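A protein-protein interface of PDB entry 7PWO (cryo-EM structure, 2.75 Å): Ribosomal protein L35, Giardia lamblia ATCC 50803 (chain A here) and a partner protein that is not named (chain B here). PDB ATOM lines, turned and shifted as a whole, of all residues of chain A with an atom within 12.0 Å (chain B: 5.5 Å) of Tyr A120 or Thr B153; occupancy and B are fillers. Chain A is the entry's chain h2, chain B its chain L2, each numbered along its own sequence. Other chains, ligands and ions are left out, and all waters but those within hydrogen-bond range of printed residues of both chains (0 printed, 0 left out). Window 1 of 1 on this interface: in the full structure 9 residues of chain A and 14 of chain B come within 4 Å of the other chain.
Among the printed residues, merely in contact across the chains: Phe A115 with Gln B121, Leu A118 with Ile B154, Tyr A120 with Cys B78, Tyr A120 with Pro B79, Tyr A120 with Gln B121, Tyr A120 with Ile B122, Tyr A120 with Gly B123, Tyr A120 with Thr B153, Ala A121 with Pro B77, Ala A121 with Val B152, Val A122 with Pro B79, Val A122 with Tyr B148 and Lys A123 with Lys B151.
Lys A117 touches none of the printed residues of chain B. Printed residues of chain B within 4 Å of Lys A119: Phe B155. Of chain B, only Pro B77, Cys B78, Pro B79, Gln B121, Ile B122, Gly B123 and Thr B153 come within 4 Å of Tyr A120. Of the printed residues of chain B, Ala A121 touches Pro B77 (3.99 Å), Val B152 (3.8 Å) and Thr B153 (3.1 Å). Of the printed residues of chain B, Val A122 touches Pro B79 and Tyr B148. Of the printed residues of chain B, Lys A123 touches Lys B151. Of chain A, only Tyr A120 comes within 4 Å of Cys B78. Lys B82 touches none of the printed residues of chain A. Printed residues of chain A within 4 Å of Gln B121: Phe A115, Pro A116 and Tyr A120. Ile B122 touches one residue of chain A. Of chain A, only Ala A121 (3.8 Å) comes within 4 Å of Val B152. Thr B153 touches just these residues of chain A: Tyr A120 (3.2 Å) and Ala A121 (3.1 Å). Of chain A, only Lys A119 comes within 4 Å of Phe B155. The nearest printed residue of chain A that does not touch Thr B153 is Lys A119 (4.9 Å). The nearest printed residue of chain B that does not touch Val A122 is Val B152 (4.3 Å).
O of Pro A116 lies close to OE1 of Gln B121 (3.2 Å). The backbone carbonyl oxygen (O) of Val A124 is in hydrogen-bond range of the side-chain amino group (NZ) of Lys B151, 2.4 Å away. The backbone NH (N) of Ala A121 is in hydrogen-bond range of the backbone carbonyl oxygen (O) of Thr B153 (3.1 Å). O of Lys A119 is in hydrogen-bond range of N of Phe B155, at 3.0 Å. The backbone carbonyl oxygen (O) of Pro B77 lies close to the backbone carbonyl oxygen (O) of Tyr A120.
Hydrophobic or aromatic side chains of chain B that line the printed part of chain A: Pro B79, Tyr B148, Val B152, Ile B154 and Phe B155. Along chain B the printed residues that touch a printed residue of chain A span positions 77 to 155. Of the 10 printed residues of chain A, 9 touch a printed residue of chain B. Among the printed residues, 18 pairs touch across the chains.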
ATOM      1  N   PHE A 115     -15.282   3.035  28.547  1.00  0.00           N
ATOM      2  CA  PHE A 115     -15.891   4.246  27.989  1.00  0.00           C
ATOM      3  C   PHE A 115     -17.076   4.002  27.045  1.00  0.00           C
ATOM      4  O   PHE A 115     -16.957   4.137  25.822  1.00  0.00           O
ATOM      5  CB  PHE A 115     -14.812   5.168  27.381  1.00  0.00           C
ATOM      6  CG  PHE A 115     -14.017   4.587  26.224  1.00  0.00           C
ATOM      7  CD1 PHE A 115     -12.839   3.890  26.483  1.00  0.00           C
ATOM      8  CD2 PHE A 115     -14.398   4.767  24.910  1.00  0.00           C
ATOM      9  CE1 PHE A 115     -12.072   3.380  25.466  1.00  0.00           C
ATOM     10  CE2 PHE A 115     -13.635   4.241  23.871  1.00  0.00           C
ATOM     11  CZ  PHE A 115     -12.469   3.543  24.155  1.00  0.00           C
ATOM     12  N   PRO A 116     -18.242   3.632  27.579  1.00  0.00           N
ATOM     13  CA  PRO A 116     -19.456   3.603  26.750  1.00  0.00           C
ATOM     14  C   PRO A 116     -20.000   4.987  26.405  1.00  0.00           C
ATOM     15  O   PRO A 116     -19.335   6.003  26.612  1.00  0.00           O
ATOM     16  CB  PRO A 116     -20.450   2.801  27.602  1.00  0.00           C
ATOM     17  CG  PRO A 116     -19.902   2.807  28.972  1.00  0.00           C
ATOM     18  CD  PRO A 116     -18.428   2.944  28.867  1.00  0.00           C
ATOM     19  N   LYS A 117     -21.199   5.012  25.826  1.00  0.00           N
ATOM     20  CA  LYS A 117     -21.831   6.228  25.330  1.00  0.00           C
ATOM     21  C   LYS A 117     -22.330   7.103  26.477  1.00  0.00           C
ATOM     22  O   LYS A 117     -22.632   6.617  27.570  1.00  0.00           O
ATOM     23  CB  LYS A 117     -22.987   5.849  24.406  1.00  0.00           C
ATOM     24  CG  LYS A 117     -23.484   6.940  23.499  1.00  0.00           C
ATOM     25  CD  LYS A 117     -24.521   6.385  22.552  1.00  0.00           C
ATOM     26  CE  LYS A 117     -24.050   6.460  21.103  1.00  0.00           C
ATOM     27  NZ  LYS A 117     -25.205   6.446  20.170  1.00  0.00           N
ATOM     28  N   LEU A 118     -22.435   8.408  26.215  1.00  0.00           N
ATOM     29  CA  LEU A 118     -22.691   9.391  27.262  1.00  0.00           C
ATOM     30  C   LEU A 118     -23.523  10.551  26.722  1.00  0.00           C
ATOM     31  O   LEU A 118     -23.287  11.022  25.609  1.00  0.00           O
ATOM     32  CB  LEU A 118     -21.366   9.915  27.819  1.00  0.00           C
ATOM     33  CG  LEU A 118     -21.361  10.710  29.117  1.00  0.00           C
ATOM     34  CD1 LEU A 118     -21.310   9.770  30.303  1.00  0.00           C
ATOM     35  CD2 LEU A 118     -20.191  11.670  29.122  1.00  0.00           C
ATOM     36  N   LYS A 119     -24.475  11.028  27.523  1.00  0.00           N
ATOM     37  CA  LYS A 119     -25.283  12.188  27.159  1.00  0.00           C
ATOM     38  C   LYS A 119     -24.684  13.436  27.800  1.00  0.00           C
ATOM     39  O   LYS A 119     -24.432  13.451  29.007  1.00  0.00           O
ATOM     40  CB  LYS A 119     -26.745  12.038  27.594  1.00  0.00           C
ATOM     41  CG  LYS A 119     -27.511  10.897  26.940  1.00  0.00           C
ATOM     42  CD  LYS A 119     -28.990  10.886  27.374  1.00  0.00           C
ATOM     43  CE  LYS A 119     -29.221  10.484  28.826  1.00  0.00           C
ATOM     44  NZ  LYS A 119     -28.869   9.077  29.152  1.00  0.00           N
ATOM     45  N   TYR A 120     -24.461  14.474  26.994  1.00  0.00           N
ATOM     46  CA  TYR A 120     -23.876  15.717  27.478  1.00  0.00           C
ATOM     47  C   TYR A 120     -24.426  16.888  26.675  1.00  0.00           C
ATOM     48  O   TYR A 120     -24.797  16.736  25.513  1.00  0.00           O
ATOM     49  CB  TYR A 120     -22.342  15.677  27.394  1.00  0.00           C
ATOM     50  CG  TYR A 120     -21.828  15.459  25.992  1.00  0.00           C
ATOM     51  CD1 TYR A 120     -21.709  16.512  25.103  1.00  0.00           C
ATOM     52  CD2 TYR A 120     -21.501  14.191  25.550  1.00  0.00           C
ATOM     53  CE1 TYR A 120     -21.272  16.308  23.827  1.00  0.00           C
ATOM     54  CE2 TYR A 120     -21.061  13.977  24.270  1.00  0.00           C
ATOM     55  CZ  TYR A 120     -20.948  15.037  23.414  1.00  0.00           C
ATOM     56  OH  TYR A 120     -20.500  14.839  22.136  1.00  0.00           O
ATOM     57  N   ALA A 121     -24.464  18.058  27.300  1.00  0.00           N
ATOM     58  CA  ALA A 121     -24.845  19.284  26.618  1.00  0.00           C
ATOM     59  C   ALA A 121     -23.653  20.228  26.544  1.00  0.00           C
ATOM     60  O   ALA A 121     -22.795  20.238  27.427  1.00  0.00           O
ATOM     61  CB  ALA A 121     -26.015  19.973  27.318  1.00  0.00           C
ATOM     62  N   VAL A 122     -23.592  21.002  25.463  1.00  0.00           N
ATOM     63  CA  VAL A 122     -22.581  22.036  25.283  1.00  0.00           C
ATOM     64  C   VAL A 122     -23.288  23.379  25.210  1.00  0.00           C
ATOM     65  O   VAL A 122     -24.252  23.536  24.454  1.00  0.00           O
ATOM     66  CB  VAL A 122     -21.719  21.808  24.024  1.00  0.00           C
ATOM     67  CG1 VAL A 122     -20.553  22.760  24.016  1.00  0.00           C
ATOM     68  CG2 VAL A 122     -21.213  20.375  23.948  1.00  0.00           C
ATOM     69  N   LYS A 123     -22.802  24.344  25.982  1.00  0.00           N
ATOM     70  CA  LYS A 123     -23.406  25.662  26.075  1.00  0.00           C
ATOM     71  C   LYS A 123     -22.697  26.645  25.146  1.00  0.00           C
ATOM     72  O   LYS A 123     -21.724  26.316  24.467  1.00  0.00           O
ATOM     73  CB  LYS A 123     -23.375  26.154  27.521  1.00  0.00           C
ATOM     74  CG  LYS A 123     -24.341  25.427  28.425  1.00  0.00           C
ATOM     75  CD  LYS A 123     -25.700  26.114  28.440  1.00  0.00           C
ATOM     76  CE  LYS A 123     -26.513  25.701  29.656  1.00  0.00           C
ATOM     77  NZ  LYS A 123     -27.089  24.345  29.462  1.00  0.00           N
ATOM     78  N   VAL A 124     -23.211  27.869  25.100  1.00  0.00           N
ATOM     79  CA  VAL A 124     -22.560  28.934  24.348  1.00  0.00           C
ATOM     80  C   VAL A 124     -21.684  29.752  25.282  1.00  0.00           C
ATOM     81  O   VAL A 124     -21.556  29.432  26.459  1.00  0.00           O
ATOM     82  CB  VAL A 124     -23.578  29.831  23.634  1.00  0.00           C
ATOM     83  CG1 VAL A 124     -24.144  29.123  22.416  1.00  0.00           C
ATOM     84  CG2 VAL A 124     -24.695  30.257  24.603  1.00  0.00           C
ATOM     85  N   PRO B  77     -29.500  15.541  24.113  1.00  0.00           N
ATOM     86  CA  PRO B  77     -29.218  16.932  23.744  1.00  0.00           C
ATOM     87  C   PRO B  77     -27.784  17.165  23.299  1.00  0.00           C
ATOM     88  O   PRO B  77     -27.212  18.215  23.589  1.00  0.00           O
ATOM     89  CB  PRO B  77     -29.500  17.696  25.041  1.00  0.00           C
ATOM     90  CG  PRO B  77     -29.205  16.711  26.134  1.00  0.00           C
ATOM     91  CD  PRO B  77     -29.146  15.303  25.519  1.00  0.00           C
ATOM     92  N   CYS B  78     -27.204  16.191  22.611  1.00  0.00           N
ATOM     93  CA  CYS B  78     -25.877  16.383  22.063  1.00  0.00           C
ATOM     94  C   CYS B  78     -25.931  17.341  20.875  1.00  0.00           C
ATOM     95  O   CYS B  78     -26.959  17.458  20.207  1.00  0.00           O
ATOM     96  CB  CYS B  78     -25.274  15.052  21.627  1.00  0.00           C
ATOM     97  SG  CYS B  78     -25.462  13.713  22.809  1.00  0.00           S
ATOM     98  N   PRO B  79     -24.842  18.051  20.603  1.00  0.00           N
ATOM     99  CA  PRO B  79     -24.739  18.787  19.341  1.00  0.00           C
ATOM    100  C   PRO B  79     -24.500  17.855  18.162  1.00  0.00           C
ATOM    101  O   PRO B  79     -24.034  16.723  18.302  1.00  0.00           O
ATOM    102  CB  PRO B  79     -23.548  19.718  19.569  1.00  0.00           C
ATOM    103  CG  PRO B  79     -22.750  19.053  20.630  1.00  0.00           C
ATOM    104  CD  PRO B  79     -23.717  18.339  21.510  1.00  0.00           C
ATOM    105  N   LYS B  82     -18.826  17.722  16.392  1.00  0.00           N
ATOM    106  CA  LYS B  82     -17.737  17.517  17.334  1.00  0.00           C
ATOM    107  C   LYS B  82     -16.944  18.809  17.519  1.00  0.00           C
ATOM    108  O   LYS B  82     -16.998  19.721  16.696  1.00  0.00           O
ATOM    109  CB  LYS B  82     -16.811  16.412  16.835  1.00  0.00           C
ATOM    110  CG  LYS B  82     -17.511  15.130  16.441  1.00  0.00           C
ATOM    111  CD  LYS B  82     -18.467  14.660  17.519  1.00  0.00           C
ATOM    112  CE  LYS B  82     -18.453  13.148  17.621  1.00  0.00           C
ATOM    113  NZ  LYS B  82     -19.043  12.695  18.906  1.00  0.00           N
ATOM    114  N   GLN B 121     -15.061  10.148  23.956  1.00  0.00           N
ATOM    115  CA  GLN B 121     -16.318   9.937  24.663  1.00  0.00           C
ATOM    116  C   GLN B 121     -17.017  11.251  24.984  1.00  0.00           C
ATOM    117  O   GLN B 121     -18.229  11.380  24.784  1.00  0.00           O
ATOM    118  CB  GLN B 121     -16.063   9.144  25.940  1.00  0.00           C
ATOM    119  CG  GLN B 121     -17.139   9.288  26.983  1.00  0.00           C
ATOM    120  CD  GLN B 121     -16.801   8.542  28.243  1.00  0.00           C
ATOM    121  OE1 GLN B 121     -17.097   7.358  28.378  1.00  0.00           O
ATOM    122  NE2 GLN B 121     -16.144   9.227  29.172  1.00  0.00           N
ATOM    123  N   ILE B 122     -16.282  12.243  25.489  1.00  0.00           N
ATOM    124  CA  ILE B 122     -16.963  13.487  25.860  1.00  0.00           C
ATOM    125  C   ILE B 122     -17.125  14.429  24.673  1.00  0.00           C
ATOM    126  O   ILE B 122     -17.558  15.573  24.841  1.00  0.00           O
ATOM    127  CB  ILE B 122     -16.260  14.217  27.015  1.00  0.00           C
ATOM    128  CG1 ILE B 122     -14.787  14.444  26.699  1.00  0.00           C
ATOM    129  CG2 ILE B 122     -16.474  13.479  28.326  1.00  0.00           C
ATOM    130  CD1 ILE B 122     -14.066  15.163  27.781  1.00  0.00           C
ATOM    131  N   GLY B 123     -16.765  13.976  23.478  1.00  0.00           N
ATOM    132  CA  GLY B 123     -17.230  14.646  22.279  1.00  0.00           C
ATOM    133  C   GLY B 123     -16.242  15.523  21.549  1.00  0.00           C
ATOM    134  O   GLY B 123     -16.602  16.587  21.044  1.00  0.00           O
ATOM    135  N   TYR B 148     -13.530  24.749  26.339  1.00  0.00           N
ATOM    136  CA  TYR B 148     -14.625  23.825  26.054  1.00  0.00           C
ATOM    137  C   TYR B 148     -14.943  22.947  27.261  1.00  0.00           C
ATOM    138  O   TYR B 148     -16.110  22.819  27.661  1.00  0.00           O
ATOM    139  CB  TYR B 148     -14.259  22.962  24.853  1.00  0.00           C
ATOM    140  CG  TYR B 148     -15.292  21.947  24.471  1.00  0.00           C
ATOM    141  CD1 TYR B 148     -16.531  22.339  23.979  1.00  0.00           C
ATOM    142  CD2 TYR B 148     -15.043  20.593  24.614  1.00  0.00           C
ATOM    143  CE1 TYR B 148     -17.475  21.404  23.622  1.00  0.00           C
ATOM    144  CE2 TYR B 148     -15.987  19.658  24.267  1.00  0.00           C
ATOM    145  CZ  TYR B 148     -17.194  20.065  23.768  1.00  0.00           C
ATOM    146  OH  TYR B 148     -18.124  19.118  23.426  1.00  0.00           O
ATOM    147  N   LYS B 151     -16.986  24.693  29.582  1.00  0.00           N
ATOM    148  CA  LYS B 151     -18.351  25.026  29.188  1.00  0.00           C
ATOM    149  C   LYS B 151     -19.245  23.801  28.955  1.00  0.00           C
ATOM    150  O   LYS B 151     -20.426  23.965  28.633  1.00  0.00           O
ATOM    151  CB  LYS B 151     -18.272  25.908  27.937  1.00  0.00           C
ATOM    152  CG  LYS B 151     -19.543  26.510  27.409  1.00  0.00           C
ATOM    153  CD  LYS B 151     -19.214  27.336  26.185  1.00  0.00           C
ATOM    154  CE  LYS B 151     -18.456  28.609  26.553  1.00  0.00           C
ATOM    155  NZ  LYS B 151     -19.280  29.568  27.328  1.00  0.00           N
ATOM    156  N   VAL B 152     -18.714  22.571  29.100  1.00  0.00           N
ATOM    157  CA  VAL B 152     -19.494  21.341  28.934  1.00  0.00           C
ATOM    158  C   VAL B 152     -20.121  20.899  30.252  1.00  0.00           C
ATOM    159  O   VAL B 152     -19.499  20.996  31.314  1.00  0.00           O
ATOM    160  CB  VAL B 152     -18.619  20.219  28.351  1.00  0.00           C
ATOM    161  CG1 VAL B 152     -19.378  18.925  28.286  1.00  0.00           C
ATOM    162  CG2 VAL B 152     -18.186  20.581  26.962  1.00  0.00           C
ATOM    163  N   THR B 153     -21.358  20.389  30.173  1.00  0.00           N
ATOM    164  CA  THR B 153     -22.048  19.696  31.257  1.00  0.00           C
ATOM    165  C   THR B 153     -22.341  18.253  30.857  1.00  0.00           C
ATOM    166  O   THR B 153     -22.490  17.942  29.673  1.00  0.00           O
ATOM    167  CB  THR B 153     -23.368  20.386  31.625  1.00  0.00           C
ATOM    168  OG1 THR B 153     -23.984  19.704  32.724  1.00  0.00           O
ATOM    169  CG2 THR B 153     -24.311  20.378  30.455  1.00  0.00           C
ATOM    170  N   ILE B 154     -22.428  17.370  31.850  1.00  0.00           N
ATOM    171  CA  ILE B 154     -22.584  15.935  31.622  1.00  0.00           C
ATOM    172  C   ILE B 154     -23.736  15.390  32.457  1.00  0.00           C
ATOM    173  O   ILE B 154     -23.885  15.740  33.633  1.00  0.00           O
ATOM    174  CB  ILE B 154     -21.278  15.172  31.937  1.00  0.00           C
ATOM    175  CG1 ILE B 154     -20.143  15.644  31.031  1.00  0.00           C
ATOM    176  CG2 ILE B 154     -21.472  13.680  31.795  1.00  0.00           C
ATOM    177  CD1 ILE B 154     -18.797  15.116  31.438  1.00  0.00           C
ATOM    178  N   PHE B 155     -24.552  14.534  31.849  1.00  0.00           N
ATOM    179  CA  PHE B 155     -25.597  13.821  32.571  1.00  0.00           C
ATOM    180  C   PHE B 155     -25.249  12.348  32.733  1.00  0.00           C
ATOM    181  O   PHE B 155     -25.221  11.829  33.846  1.00  0.00           O
ATOM    182  CB  PHE B 155     -26.938  13.974  31.859  1.00  0.00           C
ATOM    183  CG  PHE B 155     -27.250  15.380  31.475  1.00  0.00           C
ATOM    184  CD1 PHE B 155     -27.345  16.363  32.439  1.00  0.00           C
ATOM    185  CD2 PHE B 155     -27.393  15.733  30.152  1.00  0.00           C
ATOM    186  CE1 PHE B 155     -27.617  17.661  32.091  1.00  0.00           C
ATOM    187  CE2 PHE B 155     -27.661  17.027  29.798  1.00  0.00           C
ATOM    188  CZ  PHE B 155     -27.774  17.996  30.768  1.00  0.00           C
